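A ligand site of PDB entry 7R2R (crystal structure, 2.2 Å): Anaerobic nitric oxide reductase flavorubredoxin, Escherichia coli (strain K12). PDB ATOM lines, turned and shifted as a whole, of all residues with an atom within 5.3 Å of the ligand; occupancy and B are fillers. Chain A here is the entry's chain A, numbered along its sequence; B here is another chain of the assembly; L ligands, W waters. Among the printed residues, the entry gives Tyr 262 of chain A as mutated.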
ATOM      1  N   ASP A 259      18.076  21.973  19.838  1.00  0.00           N
ATOM      2  CA  ASP A 259      17.939  22.149  21.275  1.00  0.00           C
ATOM      3  C   ASP A 259      19.210  22.801  21.803  1.00  0.00           C
ATOM      4  O   ASP A 259      20.293  22.598  21.244  1.00  0.00           O
ATOM      5  CB  ASP A 259      17.692  20.811  21.978  1.00  0.00           C
ATOM      6  CG  ASP A 259      17.001  20.983  23.327  1.00  0.00           C
ATOM      7  OD1 ASP A 259      17.020  22.115  23.861  1.00  0.00           O
ATOM      8  OD2 ASP A 259      16.438  20.000  23.839  1.00  0.00           O
ATOM      9  N   THR A 260      19.086  23.579  22.871  1.00  0.00           N
ATOM     10  CA  THR A 260      20.213  24.335  23.386  1.00  0.00           C
ATOM     11  C   THR A 260      20.138  24.499  24.904  1.00  0.00           C
ATOM     12  O   THR A 260      19.062  24.416  25.496  1.00  0.00           O
ATOM     13  CB  THR A 260      20.301  25.730  22.729  1.00  0.00           C
ATOM     14  OG1 THR A 260      21.490  26.397  23.165  1.00  0.00           O
ATOM     15  CG2 THR A 260      19.080  26.571  23.091  1.00  0.00           C
ATOM     16  N   MET A 261      21.291  24.734  25.521  1.00  0.00           N
ATOM     17  CA  MET A 261      21.353  24.953  26.969  1.00  0.00           C
ATOM     18  C   MET A 261      21.661  26.412  27.297  1.00  0.00           C
ATOM     19  O   MET A 261      21.136  26.954  28.274  1.00  0.00           O
ATOM     20  CB  MET A 261      22.397  24.040  27.614  1.00  0.00           C
ATOM     21  CG  MET A 261      22.140  22.546  27.405  1.00  0.00           C
ATOM     22  SD  MET A 261      23.316  21.510  28.309  1.00  0.00           S
ATOM     23  CE  MET A 261      24.765  21.665  27.267  1.00  0.00           C
ATOM     24  N   TYR A 262      22.502  27.045  26.485  1.00  0.00           N
ATOM     25  CA  TYR A 262      22.904  28.429  26.719  1.00  0.00           C
ATOM     26  C   TYR A 262      22.789  29.290  25.467  1.00  0.00           C
ATOM     27  O   TYR A 262      23.480  30.299  25.341  1.00  0.00           O
ATOM     28  CB  TYR A 262      24.337  28.477  27.260  1.00  0.00           C
ATOM     29  CG  TYR A 262      24.508  27.761  28.576  1.00  0.00           C
ATOM     30  CD1 TYR A 262      23.903  28.244  29.732  1.00  0.00           C
ATOM     31  CD2 TYR A 262      25.261  26.594  28.660  1.00  0.00           C
ATOM     32  CE1 TYR A 262      24.058  27.598  30.934  1.00  0.00           C
ATOM     33  CE2 TYR A 262      25.414  25.933  29.880  1.00  0.00           C
ATOM     34  CZ  TYR A 262      24.808  26.438  31.007  1.00  0.00           C
ATOM     35  OH  TYR A 262      24.956  25.798  32.214  1.00  0.00           O
ATOM     36  N   ASN A 263      21.920  28.865  24.547  1.00  0.00           N
ATOM     37  CA  ASN A 263      21.579  29.629  23.339  1.00  0.00           C
ATOM     38  C   ASN A 263      22.709  29.791  22.312  1.00  0.00           C
ATOM     39  O   ASN A 263      22.562  30.544  21.350  1.00  0.00           O
ATOM     40  CB  ASN A 263      21.047  31.010  23.723  1.00  0.00           C
ATOM     41  CG  ASN A 263      19.744  30.934  24.502  1.00  0.00           C
ATOM     42  OD1 ASN A 263      18.691  30.630  23.942  1.00  0.00           O
ATOM     43  ND2 ASN A 263      19.824  31.208  25.797  1.00  0.00           N
ATOM     44  N   ASN A 264      23.812  29.088  22.512  1.00  0.00           N
ATOM     45  CA  ASN A 264      24.915  29.144  21.561  1.00  0.00           C
ATOM     46  C   ASN A 264      24.521  28.557  20.204  1.00  0.00           C
ATOM     47  O   ASN A 264      24.779  29.145  19.163  1.00  0.00           O
ATOM     48  CB  ASN A 264      26.150  28.432  22.110  1.00  0.00           C
ATOM     49  CG  ASN A 264      26.756  29.167  23.297  1.00  0.00           C
ATOM     50  OD1 ASN A 264      27.393  28.560  24.159  1.00  0.00           O
ATOM     51  ND2 ASN A 264      26.550  30.473  23.353  1.00  0.00           N
ATOM     52  N   THR A 265      23.887  27.380  20.239  1.00  0.00           N
ATOM     53  CA  THR A 265      23.411  26.726  19.025  1.00  0.00           C
ATOM     54  C   THR A 265      22.273  27.514  18.385  1.00  0.00           C
ATOM     55  O   THR A 265      22.135  27.560  17.159  1.00  0.00           O
ATOM     56  CB  THR A 265      22.931  25.280  19.323  1.00  0.00           C
ATOM     57  OG1 THR A 265      24.030  24.522  19.847  1.00  0.00           O
ATOM     58  CG2 THR A 265      22.415  24.598  18.067  1.00  0.00           C
ATOM     59  N   ARG A 266      21.457  28.164  19.222  1.00  0.00           N
ATOM     60  CA  ARG A 266      20.381  29.005  18.733  1.00  0.00           C
ATOM     61  C   ARG A 266      20.898  30.147  17.884  1.00  0.00           C
ATOM     62  O   ARG A 266      20.357  30.450  16.815  1.00  0.00           O
ATOM     63  CB  ARG A 266      19.559  29.557  19.902  1.00  0.00           C
ATOM     64  CG  ARG A 266      18.575  30.643  19.486  1.00  0.00           C
ATOM     65  CD  ARG A 266      17.875  31.252  20.690  1.00  0.00           C
ATOM     66  NE  ARG A 266      16.905  32.261  20.285  1.00  0.00           N
ATOM     67  CZ  ARG A 266      16.022  32.820  21.099  1.00  0.00           C
ATOM     68  NH1 ARG A 266      15.979  32.461  22.387  1.00  0.00           N
ATOM     69  NH2 ARG A 266      15.172  33.730  20.647  1.00  0.00           N
ATOM     70  N   SER A 313      23.961  20.827  20.988  1.00  0.00           N
ATOM     71  CA  SER A 313      25.213  21.021  21.712  1.00  0.00           C
ATOM     72  C   SER A 313      25.716  19.669  22.200  1.00  0.00           C
ATOM     73  O   SER A 313      24.953  18.706  22.273  1.00  0.00           O
ATOM     74  CB  SER A 313      25.036  21.983  22.878  1.00  0.00           C
ATOM     75  OG  SER A 313      24.013  21.547  23.763  1.00  0.00           O
ATOM     76  N   THR A 314      27.005  19.594  22.524  1.00  0.00           N
ATOM     77  CA  THR A 314      27.570  18.368  23.047  1.00  0.00           C
ATOM     78  C   THR A 314      27.418  18.303  24.556  1.00  0.00           C
ATOM     79  O   THR A 314      27.872  19.202  25.271  1.00  0.00           O
ATOM     80  CB  THR A 314      29.055  18.206  22.659  1.00  0.00           C
ATOM     81  OG1 THR A 314      29.192  18.238  21.233  1.00  0.00           O
ATOM     82  CG2 THR A 314      29.597  16.882  23.188  1.00  0.00           C
ATOM     83  N   MET A 315      26.776  17.256  25.038  1.00  0.00           N
ATOM     84  CA  MET A 315      26.543  17.070  26.460  1.00  0.00           C
ATOM     85  C   MET A 315      26.926  15.648  26.847  1.00  0.00           C
ATOM     86  O   MET A 315      26.273  14.695  26.436  1.00  0.00           O
ATOM     87  CB  MET A 315      25.081  17.352  26.813  1.00  0.00           C
ATOM     88  CG  MET A 315      24.754  17.263  28.300  1.00  0.00           C
ATOM     89  SD  MET A 315      22.998  17.521  28.612  1.00  0.00           S
ATOM     90  CE  MET A 315      22.952  17.357  30.399  1.00  0.00           C
ATOM     91  N   ASN A 316      27.994  15.521  27.637  1.00  0.00           N
ATOM     92  CA  ASN A 316      28.549  14.215  28.010  1.00  0.00           C
ATOM     93  C   ASN A 316      28.896  13.392  26.775  1.00  0.00           C
ATOM     94  O   ASN A 316      28.572  12.208  26.698  1.00  0.00           O
ATOM     95  CB  ASN A 316      27.579  13.458  28.908  1.00  0.00           C
ATOM     96  CG  ASN A 316      27.296  14.184  30.207  1.00  0.00           C
ATOM     97  OD1 ASN A 316      28.163  14.835  30.769  1.00  0.00           O
ATOM     98  ND2 ASN A 316      26.056  14.072  30.690  1.00  0.00           N
ATOM     99  N   ASN A 317      29.532  14.041  25.804  1.00  0.00           N
ATOM    100  CA  ASN A 317      29.993  13.425  24.551  1.00  0.00           C
ATOM    101  C   ASN A 317      28.879  12.956  23.620  1.00  0.00           C
ATOM    102  O   ASN A 317      29.155  12.413  22.550  1.00  0.00           O
ATOM    103  CB  ASN A 317      30.941  12.255  24.852  1.00  0.00           C
ATOM    104  CG  ASN A 317      32.139  12.675  25.682  1.00  0.00           C
ATOM    105  OD1 ASN A 317      33.048  13.338  25.188  1.00  0.00           O
ATOM    106  ND2 ASN A 317      32.142  12.282  26.950  1.00  0.00           N
ATOM    107  N   SER A 345      27.092  23.772  18.843  1.00  0.00           N
ATOM    108  CA  SER A 345      28.238  24.277  19.599  1.00  0.00           C
ATOM    109  C   SER A 345      28.781  23.222  20.561  1.00  0.00           C
ATOM    110  O   SER A 345      28.075  22.294  20.950  1.00  0.00           O
ATOM    111  CB  SER A 345      27.838  25.534  20.373  1.00  0.00           C
ATOM    112  OG  SER A 345      28.885  25.934  21.253  1.00  0.00           O
ATOM    113  N   HIS A 346      30.046  23.379  20.940  1.00  0.00           N
ATOM    114  CA  HIS A 346      30.668  22.467  21.895  1.00  0.00           C
ATOM    115  C   HIS A 346      31.635  23.226  22.805  1.00  0.00           C
ATOM    116  O   HIS A 346      31.924  24.393  22.574  1.00  0.00           O
ATOM    117  CB  HIS A 346      31.402  21.341  21.166  1.00  0.00           C
ATOM    118  CG  HIS A 346      32.575  21.796  20.363  1.00  0.00           C
ATOM    119  ND1 HIS A 346      32.473  22.158  19.038  1.00  0.00           N
ATOM    120  CD2 HIS A 346      33.872  21.952  20.702  1.00  0.00           C
ATOM    121  CE1 HIS A 346      33.665  22.519  18.599  1.00  0.00           C
ATOM    122  NE2 HIS A 346      34.530  22.404  19.582  1.00  0.00           N
ATOM    123  N   GLY A 347      32.124  22.533  23.827  1.00  0.00           N
ATOM    124  CA  GLY A 347      33.005  23.147  24.802  1.00  0.00           C
ATOM    125  C   GLY A 347      34.463  22.820  24.589  1.00  0.00           C
ATOM    126  O   GLY A 347      35.313  23.726  24.582  1.00  0.00           O
ATOM    127  N   TRP A 348      34.777  21.542  24.412  1.00  0.00           N
ATOM    128  CA  TRP A 348      36.164  21.131  24.206  1.00  0.00           C
ATOM    129  C   TRP A 348      36.313  20.114  23.071  1.00  0.00           C
ATOM    130  O   TRP A 348      36.705  20.483  21.962  1.00  0.00           O
ATOM    131  CB  TRP A 348      36.756  20.555  25.506  1.00  0.00           C
ATOM    132  CG  TRP A 348      35.830  19.663  26.294  1.00  0.00           C
ATOM    133  CD1 TRP A 348      35.815  18.302  26.297  1.00  0.00           C
ATOM    134  CD2 TRP A 348      34.805  20.074  27.207  1.00  0.00           C
ATOM    135  NE1 TRP A 348      34.836  17.839  27.149  1.00  0.00           N
ATOM    136  CE2 TRP A 348      34.204  18.912  27.723  1.00  0.00           C
ATOM    137  CE3 TRP A 348      34.342  21.322  27.642  1.00  0.00           C
ATOM    138  CZ2 TRP A 348      33.165  18.947  28.647  1.00  0.00           C
ATOM    139  CZ3 TRP A 348      33.297  21.356  28.559  1.00  0.00           C
ATOM    140  CH2 TRP A 348      32.726  20.179  29.052  1.00  0.00           C
ATOM    141  N   SER A 349      36.010  18.850  23.340  1.00  0.00           N
ATOM    142  CA  SER A 349      36.232  17.794  22.359  1.00  0.00           C
ATOM    143  C   SER A 349      35.054  17.630  21.399  1.00  0.00           C
ATOM    144  O   SER A 349      35.226  17.177  20.260  1.00  0.00           O
ATOM    145  CB  SER A 349      36.524  16.467  23.057  1.00  0.00           C
ATOM    146  OG  SER A 349      35.486  16.121  23.954  1.00  0.00           O
ATOM    147  N   GLY A 350      33.854  18.007  21.848  1.00  0.00           N
ATOM    148  CA  GLY A 350      32.664  17.883  21.037  1.00  0.00           C
ATOM    149  C   GLY A 350      32.362  16.454  20.635  1.00  0.00           C
ATOM    150  O   GLY A 350      32.670  15.524  21.383  1.00  0.00           O
ATOM    151  N   LYS A 374      32.751  26.795  18.665  1.00  0.00           N
ATOM    152  CA  LYS A 374      33.197  26.615  20.046  1.00  0.00           C
ATOM    153  C   LYS A 374      32.622  27.695  20.950  1.00  0.00           C
ATOM    154  O   LYS A 374      32.748  28.892  20.668  1.00  0.00           O
ATOM    155  CB  LYS A 374      34.726  26.622  20.108  1.00  0.00           C
ATOM    156  CG  LYS A 374      35.292  26.134  21.430  1.00  0.00           C
ATOM    157  CD  LYS A 374      36.817  26.126  21.419  1.00  0.00           C
ATOM    158  CE  LYS A 374      37.372  25.600  22.730  1.00  0.00           C
ATOM    159  NZ  LYS A 374      38.859  25.585  22.738  1.00  0.00           N
ATOM    160  N   TRP A 375      31.984  27.276  22.035  1.00  0.00           N
ATOM    161  CA  TRP A 375      31.329  28.176  22.993  1.00  0.00           C
ATOM    162  C   TRP A 375      30.351  29.122  22.289  1.00  0.00           C
ATOM    163  O   TRP A 375      29.601  28.703  21.400  1.00  0.00           O
ATOM    164  CB  TRP A 375      32.367  28.970  23.785  1.00  0.00           C
ATOM    165  CG  TRP A 375      33.327  28.127  24.568  1.00  0.00           C
ATOM    166  CD1 TRP A 375      34.683  28.069  24.403  1.00  0.00           C
ATOM    167  CD2 TRP A 375      33.011  27.219  25.635  1.00  0.00           C
ATOM    168  NE1 TRP A 375      35.227  27.180  25.303  1.00  0.00           N
ATOM    169  CE2 TRP A 375      34.234  26.650  26.070  1.00  0.00           C
ATOM    170  CE3 TRP A 375      31.828  26.836  26.267  1.00  0.00           C
ATOM    171  CZ2 TRP A 375      34.286  25.714  27.111  1.00  0.00           C
ATOM    172  CZ3 TRP A 375      31.887  25.916  27.298  1.00  0.00           C
ATOM    173  CH2 TRP A 375      33.110  25.369  27.705  1.00  0.00           C
ATOM    174  N   ARG A 376      30.369  30.392  22.687  1.00  0.00           N
ATOM    175  CA  ARG A 376      29.507  31.387  22.064  1.00  0.00           C
ATOM    176  C   ARG A 376      30.177  31.980  20.824  1.00  0.00           C
ATOM    177  O   ARG A 376      31.294  32.487  20.911  1.00  0.00           O
ATOM    178  CB  ARG A 376      29.140  32.497  23.053  1.00  0.00           C
ATOM    179  CG  ARG A 376      28.166  33.521  22.493  1.00  0.00           C
ATOM    180  CD  ARG A 376      27.686  34.487  23.570  1.00  0.00           C
ATOM    181  NE  ARG A 376      28.766  35.335  24.072  1.00  0.00           N
ATOM    182  CZ  ARG A 376      29.057  36.534  23.587  1.00  0.00           C
ATOM    183  NH1 ARG A 376      28.355  37.045  22.583  1.00  0.00           N
ATOM    184  NH2 ARG A 376      30.066  37.233  24.116  1.00  0.00           N
ATOM    185  N   HIS B  23      20.336  23.616  32.196  1.00  0.00           N
ATOM    186  CA  HIS B  23      20.853  22.924  31.012  1.00  0.00           C
ATOM    187  C   HIS B  23      19.784  22.852  29.936  1.00  0.00           C
ATOM    188  O   HIS B  23      19.497  21.772  29.408  1.00  0.00           O
ATOM    189  CB  HIS B  23      21.353  21.522  31.365  1.00  0.00           C
ATOM    190  CG  HIS B  23      22.400  21.511  32.431  1.00  0.00           C
ATOM    191  ND1 HIS B  23      22.754  20.360  33.119  1.00  0.00           N
ATOM    192  CD2 HIS B  23      23.178  22.499  32.930  1.00  0.00           C
ATOM    193  CE1 HIS B  23      23.707  20.650  33.987  1.00  0.00           C
ATOM    194  NE2 HIS B  23      23.976  21.935  33.901  1.00  0.00           N
ATOM    195  N   GLU B  81      31.204  28.605  33.839  1.00  0.00           N
ATOM    196  CA  GLU B  81      29.862  28.335  33.344  1.00  0.00           C
ATOM    197  C   GLU B  81      28.984  29.533  33.647  1.00  0.00           C
ATOM    198  O   GLU B  81      29.176  30.224  34.648  1.00  0.00           O
ATOM    199  CB  GLU B  81      29.291  27.056  33.968  1.00  0.00           C
ATOM    200  CG  GLU B  81      28.030  26.543  33.296  1.00  0.00           C
ATOM    201  CD  GLU B  81      27.683  25.120  33.688  1.00  0.00           C
ATOM    202  OE1 GLU B  81      28.427  24.504  34.476  1.00  0.00           O
ATOM    203  OE2 GLU B  81      26.653  24.596  33.205  1.00  0.00           O
ATOM    204  N   HIS B 113      32.945  32.790  26.206  1.00  0.00           N
ATOM    205  CA  HIS B 113      31.629  33.334  26.557  1.00  0.00           C
ATOM    206  C   HIS B 113      31.583  34.857  26.452  1.00  0.00           C
ATOM    207  O   HIS B 113      30.567  35.427  26.028  1.00  0.00           O
ATOM    208  CB  HIS B 113      31.238  32.912  27.973  1.00  0.00           C
ATOM    209  CG  HIS B 113      31.047  31.439  28.152  1.00  0.00           C
ATOM    210  ND1 HIS B 113      32.076  30.599  28.511  1.00  0.00           N
ATOM    211  CD2 HIS B 113      29.945  30.662  28.024  1.00  0.00           C
ATOM    212  CE1 HIS B 113      31.617  29.360  28.592  1.00  0.00           C
ATOM    213  NE2 HIS B 113      30.329  29.377  28.301  1.00  0.00           N
ATOM    214  N   HIS B 147      33.140  19.665  37.017  1.00  0.00           N
ATOM    215  CA  HIS B 147      32.718  18.797  35.918  1.00  0.00           C
ATOM    216  C   HIS B 147      33.198  19.306  34.559  1.00  0.00           C
ATOM    217  O   HIS B 147      32.873  18.749  33.520  1.00  0.00           O
ATOM    218  CB  HIS B 147      31.191  18.646  35.914  1.00  0.00           C
ATOM    219  CG  HIS B 147      30.470  19.935  35.695  1.00  0.00           C
ATOM    220  ND1 HIS B 147      30.077  20.374  34.444  1.00  0.00           N
ATOM    221  CD2 HIS B 147      30.067  20.895  36.565  1.00  0.00           C
ATOM    222  CE1 HIS B 147      29.461  21.534  34.561  1.00  0.00           C
ATOM    223  NE2 HIS B 147      29.450  21.878  35.830  1.00  0.00           N
ATOM    224  N   TRP B 148      33.984  20.387  34.581  1.00  0.00           N
ATOM    225  CA  TRP B 148      34.500  20.988  33.350  1.00  0.00           C
ATOM    226  C   TRP B 148      36.021  20.972  33.343  1.00  0.00           C
ATOM    227  O   TRP B 148      36.656  20.823  34.392  1.00  0.00           O
ATOM    228  CB  TRP B 148      33.988  22.421  33.199  1.00  0.00           C
ATOM    229  CG  TRP B 148      32.698  22.551  32.436  1.00  0.00           C
ATOM    230  CD1 TRP B 148      31.811  21.555  32.160  1.00  0.00           C
ATOM    231  CD2 TRP B 148      32.158  23.739  31.846  1.00  0.00           C
ATOM    232  NE1 TRP B 148      30.749  22.049  31.445  1.00  0.00           N
ATOM    233  CE2 TRP B 148      30.937  23.392  31.234  1.00  0.00           C
ATOM    234  CE3 TRP B 148      32.589  25.074  31.774  1.00  0.00           C
ATOM    235  CZ2 TRP B 148      30.147  24.321  30.560  1.00  0.00           C
ATOM    236  CZ3 TRP B 148      31.808  25.991  31.107  1.00  0.00           C
ATOM    237  CH2 TRP B 148      30.595  25.608  30.508  1.00  0.00           C
ATOM    238  N   ILE B 198      24.656  14.860  37.108  1.00  0.00           N
ATOM    239  CA  ILE B 198      25.768  15.695  36.657  1.00  0.00           C
ATOM    240  C   ILE B 198      27.135  15.005  36.740  1.00  0.00           C
ATOM    241  O   ILE B 198      27.880  14.983  35.771  1.00  0.00           O
ATOM    242  CB  ILE B 198      25.846  17.016  37.443  1.00  0.00           C
ATOM    243  CG1 ILE B 198      24.495  17.744  37.420  1.00  0.00           C
ATOM    244  CG2 ILE B 198      26.953  17.908  36.910  1.00  0.00           C
ATOM    245  CD1 ILE B 198      23.981  18.005  36.033  1.00  0.00           C
HETATM  246  N1  LIG L   1      31.360  20.295  25.607  1.00  0.00           N
HETATM  247  C1  LIG L   1      32.071  19.323  24.928  1.00  0.00           C
HETATM  248  O1  LIG L   1      32.824  19.639  24.010  1.00  0.00           O
HETATM  249  N2  LIG L   1      31.946  17.989  25.281  1.00  0.00           N
HETATM  250  C2  LIG L   1      31.098  17.633  26.310  1.00  0.00           C
HETATM  251  O2  LIG L   1      30.997  16.441  26.623  1.00  0.00           O
HETATM  252  C3  LIG L   1      30.383  18.597  26.993  1.00  0.00           C
HETATM  253  N3  LIG L   1      29.541  18.242  28.030  1.00  0.00           N
HETATM  254  C4  LIG L   1      28.825  19.213  28.701  1.00  0.00           C
HETATM  255  C5  LIG L   1      27.979  18.850  29.742  1.00  0.00           C
HETATM  256  C6  LIG L   1      27.258  19.813  30.418  1.00  0.00           C
HETATM  257  C7  LIG L   1      26.345  19.409  31.547  1.00  0.00           C
HETATM  258  C8  LIG L   1      27.383  21.154  30.077  1.00  0.00           C
HETATM  259  C9  LIG L   1      26.615  22.209  30.806  1.00  0.00           C
HETATM  260  C10 LIG L   1      28.229  21.517  29.036  1.00  0.00           C
HETATM  261  C11 LIG L   1      28.954  20.555  28.344  1.00  0.00           C
HETATM  262  N4  LIG L   1      29.795  20.910  27.307  1.00  0.00           N
HETATM  263  C12 LIG L   1      30.512  19.939  26.636  1.00  0.00           C
HETATM  264  C13 LIG L   1      29.956  22.351  26.910  1.00  0.00           C
HETATM  265  C14 LIG L   1      28.882  22.809  25.922  1.00  0.00           C
HETATM  266  O3  LIG L   1      28.884  21.988  24.779  1.00  0.00           O
HETATM  267  C15 LIG L   1      29.140  24.267  25.533  1.00  0.00           C
HETATM  268  O4  LIG L   1      28.864  25.096  26.643  1.00  0.00           O
HETATM  269  C16 LIG L   1      28.280  24.715  24.342  1.00  0.00           C
HETATM  270  O5  LIG L   1      28.916  25.791  23.705  1.00  0.00           O
HETATM  271  C17 LIG L   1      26.887  25.144  24.775  1.00  0.00           C
HETATM  272  O6  LIG L   1      25.966  24.862  23.749  1.00  0.00           O
HETATM  273  P1  LIG L   1      24.471  25.457  23.759  1.00  0.00           P
HETATM  274  O7  LIG L   1      24.005  25.597  22.335  1.00  0.00           O
HETATM  275  O8  LIG L   1      23.567  24.526  24.520  1.00  0.00           O
HETATM  276  O9  LIG L   1      24.476  26.823  24.404  1.00  0.00           O
HETATM  277  O   HOH W   1      32.412  15.149  28.606  1.00  0.00           O
HETATM  278  O   HOH W   2      33.069  15.732  24.056  1.00  0.00           O
HETATM  279  O   HOH W   3      30.506  16.044  30.067  1.00  0.00           O
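An oxygen (O5) of the ligand lies within hydrogen-bond range of the side-chain hydroxyl of Ser 345, at 2.5 Å. The backbone NH (N) of Met 261 sits at hydrogen-bond distance from an oxygen (O8) of the ligand (2.5 Å). The backbone NH (N) of Thr 265 lies within hydrogen-bond range of an oxygen (O7) of the ligand (2.8 Å). The side-chain hydroxyl (OG1) of Thr 265 is in hydrogen-bond range of an oxygen (O7) of the ligand (2.7 Å). N of Trp 348 sits at hydrogen-bond distance from O1 of the ligand (2.8 Å). OG1 of Thr 260 lies within hydrogen-bond range of O7 of the ligand. N of Tyr 262 is in hydrogen-bond range of O9 of the ligand. The backbone NH (N) of Gly 350 is in hydrogen-bond range of an oxygen (O1) of the ligand (2.9 Å). The backbone NH (N) of Asn 317 lies within hydrogen-bond range of an oxygen (O2) of the ligand (2.9 Å). The backbone NH of Gly 347 lies within hydrogen-bond range of a nitrogen (N1) of the ligand (3.0 Å). The backbone carbonyl oxygen (O) of Thr 314 sits at hydrogen-bond distance from an oxygen (O3) of the ligand (3.0 Å). An oxygen (O9) of the ligand lies within hydrogen-bond range of the backbone NH (N) of Asn 264 (3.0 Å). OD1 of Asn 264 sits at hydrogen-bond distance from O5 of the ligand (3.2 Å). The side-chain hydroxyl (OG) of Ser 313 is in hydrogen-bond range of an oxygen (O8) of the ligand (3.1 Å). A nitrogen (N3) of the ligand lies within hydrogen-bond range of the backbone NH (N) of Asn 316, at 3.2 Å. An oxygen (O9) of the ligand sits at hydrogen-bond distance from the backbone NH (N) of Asn 263, at 3.3 Å. An oxygen (O1) of the ligand sits at hydrogen-bond distance from the backbone NH (N) of Ser 349.
The side-chain hydroxyl of Thr 265 lies within hydrogen-bond range of the backbone NH of Ser 345 (3.3 Å). The backbone NH of Thr 314 sits at hydrogen-bond distance from the backbone carbonyl oxygen of Ser 345 (3.3 Å). The backbone carbonyl oxygen (O) of Trp 375 lies within hydrogen-bond range of the side-chain hydroxyl (OG) of Ser 345. The backbone NH (N) of Asn 263 is in hydrogen-bond range of the side-chain hydroxyl (OG1) of Thr 260, at 2.9 Å. The backbone carbonyl oxygen (O) of His 346 sits at hydrogen-bond distance from the backbone NH (N) of Trp 375, at 2.9 Å. A ring nitrogen (ND1) of His 147 of chain B lies close to the indole nitrogen (NE1) of Trp 148 of chain B (3.5 Å).
Residues that only touch the ligand: Trp 375, Glu 81 of chain B, His 346, Trp 148 of chain B, Met 315 and His 23 of chain B. Of the 28 residues printed, 21 come within 4 Å of the ligand.
Water W1 bridges an oxygen (O2) of the ligand (2.8 Å) and the side-chain amide nitrogen of Asn 317 (3.3 Å). Water W2 lies within hydrogen-bond range of OG of Ser 349 (2.5 Å), OD1 of Asn 317 (2.6 Å), O of Gly 350 (2.7 Å) and N2 of the ligand (2.8 Å). Water W3 bridges the side-chain amide oxygen of Asn 316 (2.7 Å) and a nitrogen (N3) of the ligand (3.1 Å).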
